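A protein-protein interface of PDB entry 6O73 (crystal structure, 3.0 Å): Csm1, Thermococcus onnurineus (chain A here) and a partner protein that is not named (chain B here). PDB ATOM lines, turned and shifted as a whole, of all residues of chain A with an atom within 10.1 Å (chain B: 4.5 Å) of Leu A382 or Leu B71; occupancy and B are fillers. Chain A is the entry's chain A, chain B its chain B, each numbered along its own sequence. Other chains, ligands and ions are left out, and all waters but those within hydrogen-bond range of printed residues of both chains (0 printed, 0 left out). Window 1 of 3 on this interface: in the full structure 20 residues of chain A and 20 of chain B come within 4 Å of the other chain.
The backbone carbonyl oxygen of Pro B75 lies within hydrogen-bond range of a ring nitrogen (NE2) of His A375 (3.3 Å). The backbone carbonyl oxygen of Leu A382 lies within hydrogen-bond range of the backbone NH of Trp B227, 2.7 Å away. The backbone carbonyl oxygen of Arg A384 lies within hydrogen-bond range of the indole nitrogen of Trp B227, at 3.2 Å.
O of His A375 lies within hydrogen-bond range of OG1 of Thr A378 (2.9 Å). The backbone NH of Leu B71 lies within hydrogen-bond range of the backbone carbonyl oxygen of Gly B250. The backbone carbonyl oxygen (O) of Leu B226 sits at hydrogen-bond distance from the backbone NH (N) of Ile B252 (2.8 Å).
Among the printed residues, pairs that only touch across the chains: Val A379 with Pro B75 (3.98 Å), Leu A382 with Leu B71 (3.9 Å), Leu A382 with Glu B74 (3.8 Å), Leu A382 with Pro B75 (3.6 Å), Leu A382 with Leu B226 (3.5 Å), Lys A383 with Trp B227 (3.4 Å) and Gly A386 with Trp B227 (3.7 Å).
Printed residues of chain B within 4 Å of Leu A382: Leu B71 (3.9 Å), Glu B74 (3.8 Å), Pro B75 (3.6 Å), Leu B226 (3.5 Å) and Trp B227 (2.7 Å). Of chain A, only Leu A382 (3.9 Å) comes within 4 Å of Leu B71. Of chain A, only Leu A382 (3.8 Å) comes within 4 Å of Glu B74. Leu B226 touches just one residue of chain A: Leu A382. No residue of chain A comes within 4 Å of Arg B228. No residue of chain A comes within 4 Å of Ser B251. Printed residues of chain A within 4 Å of Pro B75: His A375, Val A379 and Leu A382. Of the printed residues of chain B, Val A379 touches Pro B75. Of the printed residues of chain B, Gly A386 touches Trp B227 (3.7 Å). The nearest printed residue of chain B that does not touch Leu A382 is Arg B228 (4.7 Å).
Of the 23 printed residues of chain A, 6 touch a printed residue of chain B. Hydrophobic or aromatic side chains of chain A that line the printed part of chain B: His A375, Val A379 and Leu A382. Of the 13 printed residues of chain B, 5 touch a printed residue of chain A. Printed residues of chain B that touch a printed residue of chain A: Leu B71, Glu B74, Pro B75, Leu B226 and Trp B227. Hydrophobic or aromatic side chains of chain B that line the printed part of chain A: Leu B71, Pro B75 and Trp B227. Among the printed residues, 10 pairs touch across the chains. Among the printed residues, no Asp or Glu carboxylate lies within 4 Å of a Lys or Arg side-chain nitrogen of the other chain.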
ATOM      1  N   ASP A 253     -19.063  27.797   6.986  1.00  0.00           N
ATOM      2  CA  ASP A 253     -17.696  27.971   7.541  1.00  0.00           C
ATOM      3  C   ASP A 253     -16.981  29.075   6.758  1.00  0.00           C
ATOM      4  O   ASP A 253     -17.003  29.036   5.513  1.00  0.00           O
ATOM      5  CB  ASP A 253     -16.892  26.672   7.505  1.00  0.00           C
ATOM      6  CG  ASP A 253     -15.526  26.804   8.161  1.00  0.00           C
ATOM      7  OD1 ASP A 253     -15.460  27.370   9.277  1.00  0.00           O
ATOM      8  OD2 ASP A 253     -14.536  26.358   7.547  1.00  0.00           O
ATOM      9  N   SER A 255     -13.505  30.446   5.470  1.00  0.00           N
ATOM     10  CA  SER A 255     -12.107  30.028   5.180  1.00  0.00           C
ATOM     11  C   SER A 255     -11.266  31.265   4.845  1.00  0.00           C
ATOM     12  O   SER A 255     -11.775  32.178   4.167  1.00  0.00           O
ATOM     13  CB  SER A 255     -12.026  28.966   4.105  1.00  0.00           C
ATOM     14  OG  SER A 255     -12.217  29.514   2.812  1.00  0.00           O
ATOM     15  N   TYR A 344     -13.357  33.944   2.579  1.00  0.00           N
ATOM     16  CA  TYR A 344     -14.400  33.175   1.860  1.00  0.00           C
ATOM     17  C   TYR A 344     -15.504  32.753   2.834  1.00  0.00           C
ATOM     18  O   TYR A 344     -15.303  32.832   4.067  1.00  0.00           O
ATOM     19  CB  TYR A 344     -13.777  31.937   1.222  1.00  0.00           C
ATOM     20  CG  TYR A 344     -14.733  31.111   0.407  1.00  0.00           C
ATOM     21  CD1 TYR A 344     -15.475  31.696  -0.603  1.00  0.00           C
ATOM     22  CD2 TYR A 344     -14.889  29.753   0.631  1.00  0.00           C
ATOM     23  CE1 TYR A 344     -16.358  30.959  -1.370  1.00  0.00           C
ATOM     24  CE2 TYR A 344     -15.757  28.997  -0.138  1.00  0.00           C
ATOM     25  CZ  TYR A 344     -16.492  29.604  -1.142  1.00  0.00           C
ATOM     26  OH  TYR A 344     -17.360  28.889  -1.911  1.00  0.00           O
ATOM     27  N   LEU A 345     -16.636  32.314   2.280  1.00  0.00           N
ATOM     28  CA  LEU A 345     -17.762  31.735   3.047  1.00  0.00           C
ATOM     29  C   LEU A 345     -18.340  30.544   2.276  1.00  0.00           C
ATOM     30  O   LEU A 345     -19.005  30.756   1.236  1.00  0.00           O
ATOM     31  CB  LEU A 345     -18.797  32.836   3.286  1.00  0.00           C
ATOM     32  CG  LEU A 345     -19.858  32.534   4.344  1.00  0.00           C
ATOM     33  CD1 LEU A 345     -19.223  32.194   5.687  1.00  0.00           C
ATOM     34  CD2 LEU A 345     -20.812  33.710   4.486  1.00  0.00           C
ATOM     35  N   ALA A 346     -18.061  29.337   2.773  1.00  0.00           N
ATOM     36  CA  ALA A 346     -18.555  28.051   2.239  1.00  0.00           C
ATOM     37  C   ALA A 346     -19.847  27.684   2.971  1.00  0.00           C
ATOM     38  O   ALA A 346     -19.762  27.219   4.123  1.00  0.00           O
ATOM     39  CB  ALA A 346     -17.502  26.981   2.404  1.00  0.00           C
ATOM     40  N   ILE A 347     -20.992  27.916   2.327  1.00  0.00           N
ATOM     41  CA  ILE A 347     -22.338  27.545   2.851  1.00  0.00           C
ATOM     42  C   ILE A 347     -22.853  26.361   2.034  1.00  0.00           C
ATOM     43  O   ILE A 347     -23.239  26.567   0.865  1.00  0.00           O
ATOM     44  CB  ILE A 347     -23.314  28.732   2.804  1.00  0.00           C
ATOM     45  CG1 ILE A 347     -22.791  29.914   3.623  1.00  0.00           C
ATOM     46  CG2 ILE A 347     -24.698  28.287   3.253  1.00  0.00           C
ATOM     47  CD1 ILE A 347     -23.673  31.138   3.573  1.00  0.00           C
ATOM     48  N   GLU A 348     -22.823  25.174   2.633  1.00  0.00           N
ATOM     49  CA  GLU A 348     -23.492  23.963   2.106  1.00  0.00           C
ATOM     50  C   GLU A 348     -24.542  23.533   3.130  1.00  0.00           C
ATOM     51  O   GLU A 348     -24.418  23.904   4.315  1.00  0.00           O
ATOM     52  CB  GLU A 348     -22.462  22.878   1.797  1.00  0.00           C
ATOM     53  CG  GLU A 348     -21.708  23.135   0.502  1.00  0.00           C
ATOM     54  CD  GLU A 348     -22.474  22.820  -0.775  1.00  0.00           C
ATOM     55  OE1 GLU A 348     -22.466  23.668  -1.691  1.00  0.00           O
ATOM     56  OE2 GLU A 348     -23.068  21.723  -0.858  1.00  0.00           O
ATOM     57  N   LYS A 374     -20.169  18.072   6.326  1.00  0.00           N
ATOM     58  CA  LYS A 374     -18.716  18.350   6.454  1.00  0.00           C
ATOM     59  C   LYS A 374     -18.068  18.135   5.081  1.00  0.00           C
ATOM     60  O   LYS A 374     -17.486  19.096   4.545  1.00  0.00           O
ATOM     61  CB  LYS A 374     -18.070  17.457   7.518  1.00  0.00           C
ATOM     62  CG  LYS A 374     -16.643  17.843   7.882  1.00  0.00           C
ATOM     63  CD  LYS A 374     -16.566  19.097   8.733  1.00  0.00           C
ATOM     64  CE  LYS A 374     -15.261  19.853   8.581  1.00  0.00           C
ATOM     65  NZ  LYS A 374     -15.225  20.647   7.330  1.00  0.00           N
ATOM     66  N   HIS A 375     -18.205  16.930   4.522  1.00  0.00           N
ATOM     67  CA  HIS A 375     -17.696  16.560   3.175  1.00  0.00           C
ATOM     68  C   HIS A 375     -18.049  17.667   2.175  1.00  0.00           C
ATOM     69  O   HIS A 375     -17.113  18.228   1.577  1.00  0.00           O
ATOM     70  CB  HIS A 375     -18.249  15.200   2.736  1.00  0.00           C
ATOM     71  CG  HIS A 375     -17.696  14.716   1.437  1.00  0.00           C
ATOM     72  ND1 HIS A 375     -18.436  14.721   0.269  1.00  0.00           N
ATOM     73  CD2 HIS A 375     -16.483  14.215   1.115  1.00  0.00           C
ATOM     74  CE1 HIS A 375     -17.703  14.241  -0.716  1.00  0.00           C
ATOM     75  NE2 HIS A 375     -16.501  13.922  -0.223  1.00  0.00           N
ATOM     76  N   LYS A 376     -19.343  17.978   2.017  1.00  0.00           N
ATOM     77  CA  LYS A 376     -19.845  19.003   1.060  1.00  0.00           C
ATOM     78  C   LYS A 376     -19.087  20.322   1.264  1.00  0.00           C
ATOM     79  O   LYS A 376     -18.795  20.985   0.248  1.00  0.00           O
ATOM     80  CB  LYS A 376     -21.348  19.253   1.219  1.00  0.00           C
ATOM     81  CG  LYS A 376     -22.249  18.102   0.805  1.00  0.00           C
ATOM     82  CD  LYS A 376     -23.652  18.548   0.464  1.00  0.00           C
ATOM     83  CE  LYS A 376     -24.703  17.514   0.807  1.00  0.00           C
ATOM     84  NZ  LYS A 376     -24.524  16.259   0.036  1.00  0.00           N
ATOM     85  N   LEU A 377     -18.784  20.685   2.517  1.00  0.00           N
ATOM     86  CA  LEU A 377     -18.024  21.921   2.850  1.00  0.00           C
ATOM     87  C   LEU A 377     -16.577  21.813   2.348  1.00  0.00           C
ATOM     88  O   LEU A 377     -16.113  22.780   1.716  1.00  0.00           O
ATOM     89  CB  LEU A 377     -18.051  22.174   4.361  1.00  0.00           C
ATOM     90  CG  LEU A 377     -19.356  22.743   4.904  1.00  0.00           C
ATOM     91  CD1 LEU A 377     -19.391  22.645   6.418  1.00  0.00           C
ATOM     92  CD2 LEU A 377     -19.549  24.181   4.455  1.00  0.00           C
ATOM     93  N   THR A 378     -15.880  20.704   2.621  1.00  0.00           N
ATOM     94  CA  THR A 378     -14.438  20.562   2.279  1.00  0.00           C
ATOM     95  C   THR A 378     -14.274  20.680   0.756  1.00  0.00           C
ATOM     96  O   THR A 378     -13.248  21.234   0.321  1.00  0.00           O
ATOM     97  CB  THR A 378     -13.802  19.282   2.844  1.00  0.00           C
ATOM     98  OG1 THR A 378     -14.230  18.153   2.084  1.00  0.00           O
ATOM     99  CG2 THR A 378     -14.101  19.054   4.310  1.00  0.00           C
ATOM    100  N   VAL A 379     -15.249  20.207  -0.027  1.00  0.00           N
ATOM    101  CA  VAL A 379     -15.225  20.317  -1.515  1.00  0.00           C
ATOM    102  C   VAL A 379     -15.409  21.789  -1.893  1.00  0.00           C
ATOM    103  O   VAL A 379     -14.646  22.276  -2.747  1.00  0.00           O
ATOM    104  CB  VAL A 379     -16.290  19.439  -2.200  1.00  0.00           C
ATOM    105  CG1 VAL A 379     -16.304  19.656  -3.710  1.00  0.00           C
ATOM    106  CG2 VAL A 379     -16.099  17.964  -1.877  1.00  0.00           C
ATOM    107  N   ARG A 380     -16.401  22.458  -1.301  1.00  0.00           N
ATOM    108  CA  ARG A 380     -16.730  23.882  -1.580  1.00  0.00           C
ATOM    109  C   ARG A 380     -15.541  24.770  -1.194  1.00  0.00           C
ATOM    110  O   ARG A 380     -15.242  25.709  -1.955  1.00  0.00           O
ATOM    111  CB  ARG A 380     -18.001  24.301  -0.837  1.00  0.00           C
ATOM    112  CG  ARG A 380     -18.222  25.806  -0.760  1.00  0.00           C
ATOM    113  CD  ARG A 380     -18.656  26.375  -2.090  1.00  0.00           C
ATOM    114  NE  ARG A 380     -19.805  25.652  -2.612  1.00  0.00           N
ATOM    115  CZ  ARG A 380     -20.125  25.540  -3.898  1.00  0.00           C
ATOM    116  NH1 ARG A 380     -19.377  26.106  -4.834  1.00  0.00           N
ATOM    117  NH2 ARG A 380     -21.197  24.848  -4.240  1.00  0.00           N
ATOM    118  N   LYS A 381     -14.882  24.492  -0.067  1.00  0.00           N
ATOM    119  CA  LYS A 381     -13.689  25.268   0.365  1.00  0.00           C
ATOM    120  C   LYS A 381     -12.555  25.053  -0.648  1.00  0.00           C
ATOM    121  O   LYS A 381     -11.720  25.966  -0.787  1.00  0.00           O
ATOM    122  CB  LYS A 381     -13.261  24.891   1.784  1.00  0.00           C
ATOM    123  CG  LYS A 381     -14.278  25.189   2.874  1.00  0.00           C
ATOM    124  CD  LYS A 381     -13.671  25.079   4.257  1.00  0.00           C
ATOM    125  CE  LYS A 381     -14.449  24.189   5.204  1.00  0.00           C
ATOM    126  NZ  LYS A 381     -13.736  24.028   6.493  1.00  0.00           N
ATOM    127  N   LEU A 382     -12.540  23.904  -1.338  1.00  0.00           N
ATOM    128  CA  LEU A 382     -11.646  23.621  -2.499  1.00  0.00           C
ATOM    129  C   LEU A 382     -12.222  24.218  -3.795  1.00  0.00           C
ATOM    130  O   LEU A 382     -11.663  23.921  -4.870  1.00  0.00           O
ATOM    131  CB  LEU A 382     -11.472  22.107  -2.666  1.00  0.00           C
ATOM    132  CG  LEU A 382     -10.587  21.404  -1.640  1.00  0.00           C
ATOM    133  CD1 LEU A 382     -10.759  19.898  -1.748  1.00  0.00           C
ATOM    134  CD2 LEU A 382      -9.125  21.782  -1.820  1.00  0.00           C
ATOM    135  N   LYS A 383     -13.309  24.992  -3.719  1.00  0.00           N
ATOM    136  CA  LYS A 383     -13.938  25.666  -4.890  1.00  0.00           C
ATOM    137  C   LYS A 383     -14.187  27.128  -4.527  1.00  0.00           C
ATOM    138  O   LYS A 383     -15.308  27.621  -4.765  1.00  0.00           O
ATOM    139  CB  LYS A 383     -15.222  24.943  -5.308  1.00  0.00           C
ATOM    140  CG  LYS A 383     -14.977  23.606  -5.991  1.00  0.00           C
ATOM    141  CD  LYS A 383     -16.172  22.687  -6.026  1.00  0.00           C
ATOM    142  CE  LYS A 383     -16.861  22.675  -7.374  1.00  0.00           C
ATOM    143  NZ  LYS A 383     -16.063  21.946  -8.389  1.00  0.00           N
ATOM    144  N   ARG A 384     -13.165  27.780  -3.968  1.00  0.00           N
ATOM    145  CA  ARG A 384     -13.254  29.167  -3.449  1.00  0.00           C
ATOM    146  C   ARG A 384     -13.732  30.071  -4.579  1.00  0.00           C
ATOM    147  O   ARG A 384     -13.094  30.071  -5.646  1.00  0.00           O
ATOM    148  CB  ARG A 384     -11.907  29.664  -2.924  1.00  0.00           C
ATOM    149  CG  ARG A 384     -11.388  28.873  -1.738  1.00  0.00           C
ATOM    150  CD  ARG A 384     -10.184  29.537  -1.119  1.00  0.00           C
ATOM    151  NE  ARG A 384     -10.515  30.760  -0.404  1.00  0.00           N
ATOM    152  CZ  ARG A 384      -9.681  31.400   0.408  1.00  0.00           C
ATOM    153  NH1 ARG A 384      -8.461  30.931   0.609  1.00  0.00           N
ATOM    154  NH2 ARG A 384     -10.066  32.505   1.022  1.00  0.00           N
ATOM    155  N   PHE A 385     -14.843  30.768  -4.354  1.00  0.00           N
ATOM    156  CA  PHE A 385     -15.416  31.773  -5.282  1.00  0.00           C
ATOM    157  C   PHE A 385     -15.709  31.139  -6.641  1.00  0.00           C
ATOM    158  O   PHE A 385     -15.762  31.892  -7.632  1.00  0.00           O
ATOM    159  CB  PHE A 385     -14.455  32.951  -5.439  1.00  0.00           C
ATOM    160  CG  PHE A 385     -14.138  33.638  -4.141  1.00  0.00           C
ATOM    161  CD1 PHE A 385     -15.035  34.535  -3.584  1.00  0.00           C
ATOM    162  CD2 PHE A 385     -12.963  33.365  -3.463  1.00  0.00           C
ATOM    163  CE1 PHE A 385     -14.753  35.162  -2.383  1.00  0.00           C
ATOM    164  CE2 PHE A 385     -12.684  33.989  -2.258  1.00  0.00           C
ATOM    165  CZ  PHE A 385     -13.577  34.889  -1.723  1.00  0.00           C
ATOM    166  N   GLY A 386     -15.893  29.816  -6.689  1.00  0.00           N
ATOM    167  CA  GLY A 386     -16.514  29.135  -7.839  1.00  0.00           C
ATOM    168  C   GLY A 386     -17.841  29.792  -8.195  1.00  0.00           C
ATOM    169  O   GLY A 386     -18.185  29.824  -9.400  1.00  0.00           O
ATOM    170  N   GLU A 387     -18.534  30.345  -7.187  1.00  0.00           N
ATOM    171  CA  GLU A 387     -19.857  31.020  -7.308  1.00  0.00           C
ATOM    172  C   GLU A 387     -19.719  32.396  -7.974  1.00  0.00           C
ATOM    173  O   GLU A 387     -20.703  33.159  -7.944  1.00  0.00           O
ATOM    174  CB  GLU A 387     -20.508  31.198  -5.933  1.00  0.00           C
ATOM    175  CG  GLU A 387     -20.692  29.903  -5.160  1.00  0.00           C
ATOM    176  CD  GLU A 387     -19.724  29.692  -4.008  1.00  0.00           C
ATOM    177  OE1 GLU A 387     -20.117  29.031  -3.025  1.00  0.00           O
ATOM    178  OE2 GLU A 387     -18.581  30.190  -4.095  1.00  0.00           O
ATOM    179  N   LEU A 391     -14.511  35.435 -12.355  1.00  0.00           N
ATOM    180  CA  LEU A 391     -13.225  35.180 -11.651  1.00  0.00           C
ATOM    181  C   LEU A 391     -12.142  34.765 -12.655  1.00  0.00           C
ATOM    182  O   LEU A 391     -11.004  35.242 -12.505  1.00  0.00           O
ATOM    183  CB  LEU A 391     -13.416  34.104 -10.578  1.00  0.00           C
ATOM    184  CG  LEU A 391     -12.145  33.703  -9.827  1.00  0.00           C
ATOM    185  CD1 LEU A 391     -11.469  34.911  -9.194  1.00  0.00           C
ATOM    186  CD2 LEU A 391     -12.448  32.652  -8.773  1.00  0.00           C
ATOM    187  N   PHE A 392     -12.473  33.899 -13.618  1.00  0.00           N
ATOM    188  CA  PHE A 392     -11.508  33.326 -14.595  1.00  0.00           C
ATOM    189  C   PHE A 392     -11.674  34.038 -15.945  1.00  0.00           C
ATOM    190  O   PHE A 392     -12.099  33.400 -16.933  1.00  0.00           O
ATOM    191  CB  PHE A 392     -11.676  31.805 -14.663  1.00  0.00           C
ATOM    192  CG  PHE A 392     -11.620  31.126 -13.317  1.00  0.00           C
ATOM    193  CD1 PHE A 392     -10.555  31.341 -12.454  1.00  0.00           C
ATOM    194  CD2 PHE A 392     -12.639  30.281 -12.903  1.00  0.00           C
ATOM    195  CE1 PHE A 392     -10.508  30.718 -11.215  1.00  0.00           C
ATOM    196  CE2 PHE A 392     -12.593  29.664 -11.662  1.00  0.00           C
ATOM    197  CZ  PHE A 392     -11.526  29.881 -10.821  1.00  0.00           C
ATOM    198  N   LYS B  69       1.352  17.751  -3.548  1.00  0.00           N
ATOM    199  CA  LYS B  69       0.192  16.887  -3.220  1.00  0.00           C
ATOM    200  C   LYS B  69      -0.996  17.338  -4.064  1.00  0.00           C
ATOM    201  O   LYS B  69      -1.426  18.483  -3.964  1.00  0.00           O
ATOM    202  CB  LYS B  69      -0.107  16.988  -1.723  1.00  0.00           C
ATOM    203  CG  LYS B  69      -1.539  16.702  -1.317  1.00  0.00           C
ATOM    204  CD  LYS B  69      -1.996  17.609  -0.209  1.00  0.00           C
ATOM    205  CE  LYS B  69      -3.310  17.175   0.393  1.00  0.00           C
ATOM    206  NZ  LYS B  69      -3.190  15.844   1.038  1.00  0.00           N
ATOM    207  N   PRO B  70      -1.559  16.466  -4.926  1.00  0.00           N
ATOM    208  CA  PRO B  70      -2.733  16.829  -5.711  1.00  0.00           C
ATOM    209  C   PRO B  70      -3.945  17.001  -4.787  1.00  0.00           C
ATOM    210  O   PRO B  70      -4.176  16.122  -3.980  1.00  0.00           O
ATOM    211  CB  PRO B  70      -2.931  15.644  -6.661  1.00  0.00           C
ATOM    212  CG  PRO B  70      -2.268  14.478  -5.953  1.00  0.00           C
ATOM    213  CD  PRO B  70      -1.130  15.078  -5.154  1.00  0.00           C
ATOM    214  N   LEU B  71      -4.680  18.107  -4.937  1.00  0.00           N
ATOM    215  CA  LEU B  71      -5.842  18.470  -4.079  1.00  0.00           C
ATOM    216  C   LEU B  71      -6.981  17.460  -4.240  1.00  0.00           C
ATOM    217  O   LEU B  71      -7.945  17.553  -3.471  1.00  0.00           O
ATOM    218  CB  LEU B  71      -6.358  19.857  -4.463  1.00  0.00           C
ATOM    219  CG  LEU B  71      -5.421  21.033  -4.206  1.00  0.00           C
ATOM    220  CD1 LEU B  71      -6.188  22.330  -4.390  1.00  0.00           C
ATOM    221  CD2 LEU B  71      -4.804  20.958  -2.819  1.00  0.00           C
ATOM    222  N   SER B  72      -6.898  16.565  -5.223  1.00  0.00           N
ATOM    223  CA  SER B  72      -7.894  15.489  -5.463  1.00  0.00           C
ATOM    224  C   SER B  72      -7.993  14.534  -4.258  1.00  0.00           C
ATOM    225  O   SER B  72      -9.055  13.887  -4.121  1.00  0.00           O
ATOM    226  CB  SER B  72      -7.570  14.738  -6.726  1.00  0.00           C
ATOM    227  OG  SER B  72      -6.454  13.879  -6.534  1.00  0.00           O
ATOM    228  N   VAL B  73      -6.951  14.432  -3.422  1.00  0.00           N
ATOM    229  CA  VAL B  73      -6.897  13.452  -2.294  1.00  0.00           C
ATOM    230  C   VAL B  73      -7.684  13.996  -1.099  1.00  0.00           C
ATOM    231  O   VAL B  73      -8.118  13.171  -0.265  1.00  0.00           O
ATOM    232  CB  VAL B  73      -5.456  13.108  -1.874  1.00  0.00           C
ATOM    233  CG1 VAL B  73      -4.607  12.679  -3.059  1.00  0.00           C
ATOM    234  CG2 VAL B  73      -4.788  14.245  -1.117  1.00  0.00           C
ATOM    235  N   GLU B  74      -7.839  15.321  -1.011  1.00  0.00           N
ATOM    236  CA  GLU B  74      -8.434  16.013   0.164  1.00  0.00           C
ATOM    237  C   GLU B  74      -9.856  15.504   0.419  1.00  0.00           C
ATOM    238  O   GLU B  74     -10.144  15.066   1.528  1.00  0.00           O
ATOM    239  CB  GLU B  74      -8.340  17.530  -0.014  1.00  0.00           C
ATOM    240  CG  GLU B  74      -6.914  18.049   0.077  1.00  0.00           C
ATOM    241  CD  GLU B  74      -6.733  19.279   0.944  1.00  0.00           C
ATOM    242  OE1 GLU B  74      -7.389  19.355   1.993  1.00  0.00           O
ATOM    243  OE2 GLU B  74      -5.942  20.159   0.562  1.00  0.00           O
ATOM    244  N   PRO B  75     -10.799  15.516  -0.553  1.00  0.00           N
ATOM    245  CA  PRO B  75     -12.152  15.020  -0.292  1.00  0.00           C
ATOM    246  C   PRO B  75     -12.304  13.492  -0.187  1.00  0.00           C
ATOM    247  O   PRO B  75     -13.364  13.064   0.217  1.00  0.00           O
ATOM    248  CB  PRO B  75     -12.975  15.520  -1.497  1.00  0.00           C
ATOM    249  CG  PRO B  75     -12.089  16.549  -2.166  1.00  0.00           C
ATOM    250  CD  PRO B  75     -10.679  16.057  -1.916  1.00  0.00           C
ATOM    251  N   LEU B 226     -11.193  21.127  -8.614  1.00  0.00           N
ATOM    252  CA  LEU B 226     -10.780  21.492  -7.236  1.00  0.00           C
ATOM    253  C   LEU B 226      -9.594  22.448  -7.340  1.00  0.00           C
ATOM    254  O   LEU B 226      -8.807  22.302  -8.295  1.00  0.00           O
ATOM    255  CB  LEU B 226     -10.366  20.231  -6.480  1.00  0.00           C
ATOM    256  CG  LEU B 226     -11.361  19.075  -6.518  1.00  0.00           C
ATOM    257  CD1 LEU B 226     -10.729  17.825  -5.940  1.00  0.00           C
ATOM    258  CD2 LEU B 226     -12.635  19.424  -5.770  1.00  0.00           C
ATOM    259  N   TRP B 227      -9.444  23.374  -6.395  1.00  0.00           N
ATOM    260  CA  TRP B 227      -8.350  24.370  -6.472  1.00  0.00           C
ATOM    261  C   TRP B 227      -8.192  25.151  -5.172  1.00  0.00           C
ATOM    262  O   TRP B 227      -9.116  25.160  -4.338  1.00  0.00           O
ATOM    263  CB  TRP B 227      -8.594  25.315  -7.648  1.00  0.00           C
ATOM    264  CG  TRP B 227      -9.704  26.301  -7.450  1.00  0.00           C
ATOM    265  CD1 TRP B 227      -9.590  27.552  -6.920  1.00  0.00           C
ATOM    266  CD2 TRP B 227     -11.088  26.150  -7.822  1.00  0.00           C
ATOM    267  NE1 TRP B 227     -10.804  28.184  -6.926  1.00  0.00           N
ATOM    268  CE2 TRP B 227     -11.742  27.350  -7.472  1.00  0.00           C
ATOM    269  CE3 TRP B 227     -11.841  25.122  -8.405  1.00  0.00           C
ATOM    270  CZ2 TRP B 227     -13.104  27.549  -7.692  1.00  0.00           C
ATOM    271  CZ3 TRP B 227     -13.186  25.322  -8.632  1.00  0.00           C
ATOM    272  CH2 TRP B 227     -13.807  26.520  -8.275  1.00  0.00           C
ATOM    273  N   ARG B 228      -7.036  25.793  -5.043  1.00  0.00           N
ATOM    274  CA  ARG B 228      -6.799  26.895  -4.088  1.00  0.00           C
ATOM    275  C   ARG B 228      -6.365  28.109  -4.899  1.00  0.00           C
ATOM    276  O   ARG B 228      -5.447  27.967  -5.729  1.00  0.00           O
ATOM    277  CB  ARG B 228      -5.716  26.536  -3.076  1.00  0.00           C
ATOM    278  CG  ARG B 228      -6.048  25.337  -2.203  1.00  0.00           C
ATOM    279  CD  ARG B 228      -4.995  25.150  -1.127  1.00  0.00           C
ATOM    280  NE  ARG B 228      -3.705  25.726  -1.519  1.00  0.00           N
ATOM    281  CZ  ARG B 228      -2.728  25.091  -2.170  1.00  0.00           C
ATOM    282  NH1 ARG B 228      -1.613  25.737  -2.467  1.00  0.00           N
ATOM    283  NH2 ARG B 228      -2.856  23.821  -2.519  1.00  0.00           N
ATOM    284  N   GLY B 250      -1.065  22.013  -7.866  1.00  0.00           N
ATOM    285  CA  GLY B 250      -1.795  20.892  -7.242  1.00  0.00           C
ATOM    286  C   GLY B 250      -3.298  20.957  -7.473  1.00  0.00           C
ATOM    287  O   GLY B 250      -3.978  19.980  -7.120  1.00  0.00           O
ATOM    288  N   SER B 251      -3.817  22.049  -8.043  1.00  0.00           N
ATOM    289  CA  SER B 251      -5.251  22.170  -8.411  1.00  0.00           C
ATOM    290  C   SER B 251      -5.573  21.187  -9.542  1.00  0.00           C
ATOM    291  O   SER B 251      -4.630  20.738 -10.226  1.00  0.00           O
ATOM    292  CB  SER B 251      -5.614  23.574  -8.801  1.00  0.00           C
ATOM    293  OG  SER B 251      -5.108  24.515  -7.860  1.00  0.00           O
ATOM    294  N   ILE B 252      -6.859  20.893  -9.738  1.00  0.00           N
ATOM    295  CA  ILE B 252      -7.357  19.824 -10.655  1.00  0.00           C
ATOM    296  C   ILE B 252      -8.139  20.473 -11.804  1.00  0.00           C
ATOM    297  O   ILE B 252      -8.886  21.436 -11.558  1.00  0.00           O
ATOM    298  CB  ILE B 252      -8.184  18.789  -9.865  1.00  0.00           C
ATOM    299  CG1 ILE B 252      -7.442  18.337  -8.606  1.00  0.00           C
ATOM    300  CG2 ILE B 252      -8.565  17.601 -10.731  1.00  0.00           C
ATOM    301  CD1 ILE B 252      -6.118  17.654  -8.885  1.00  0.00           C
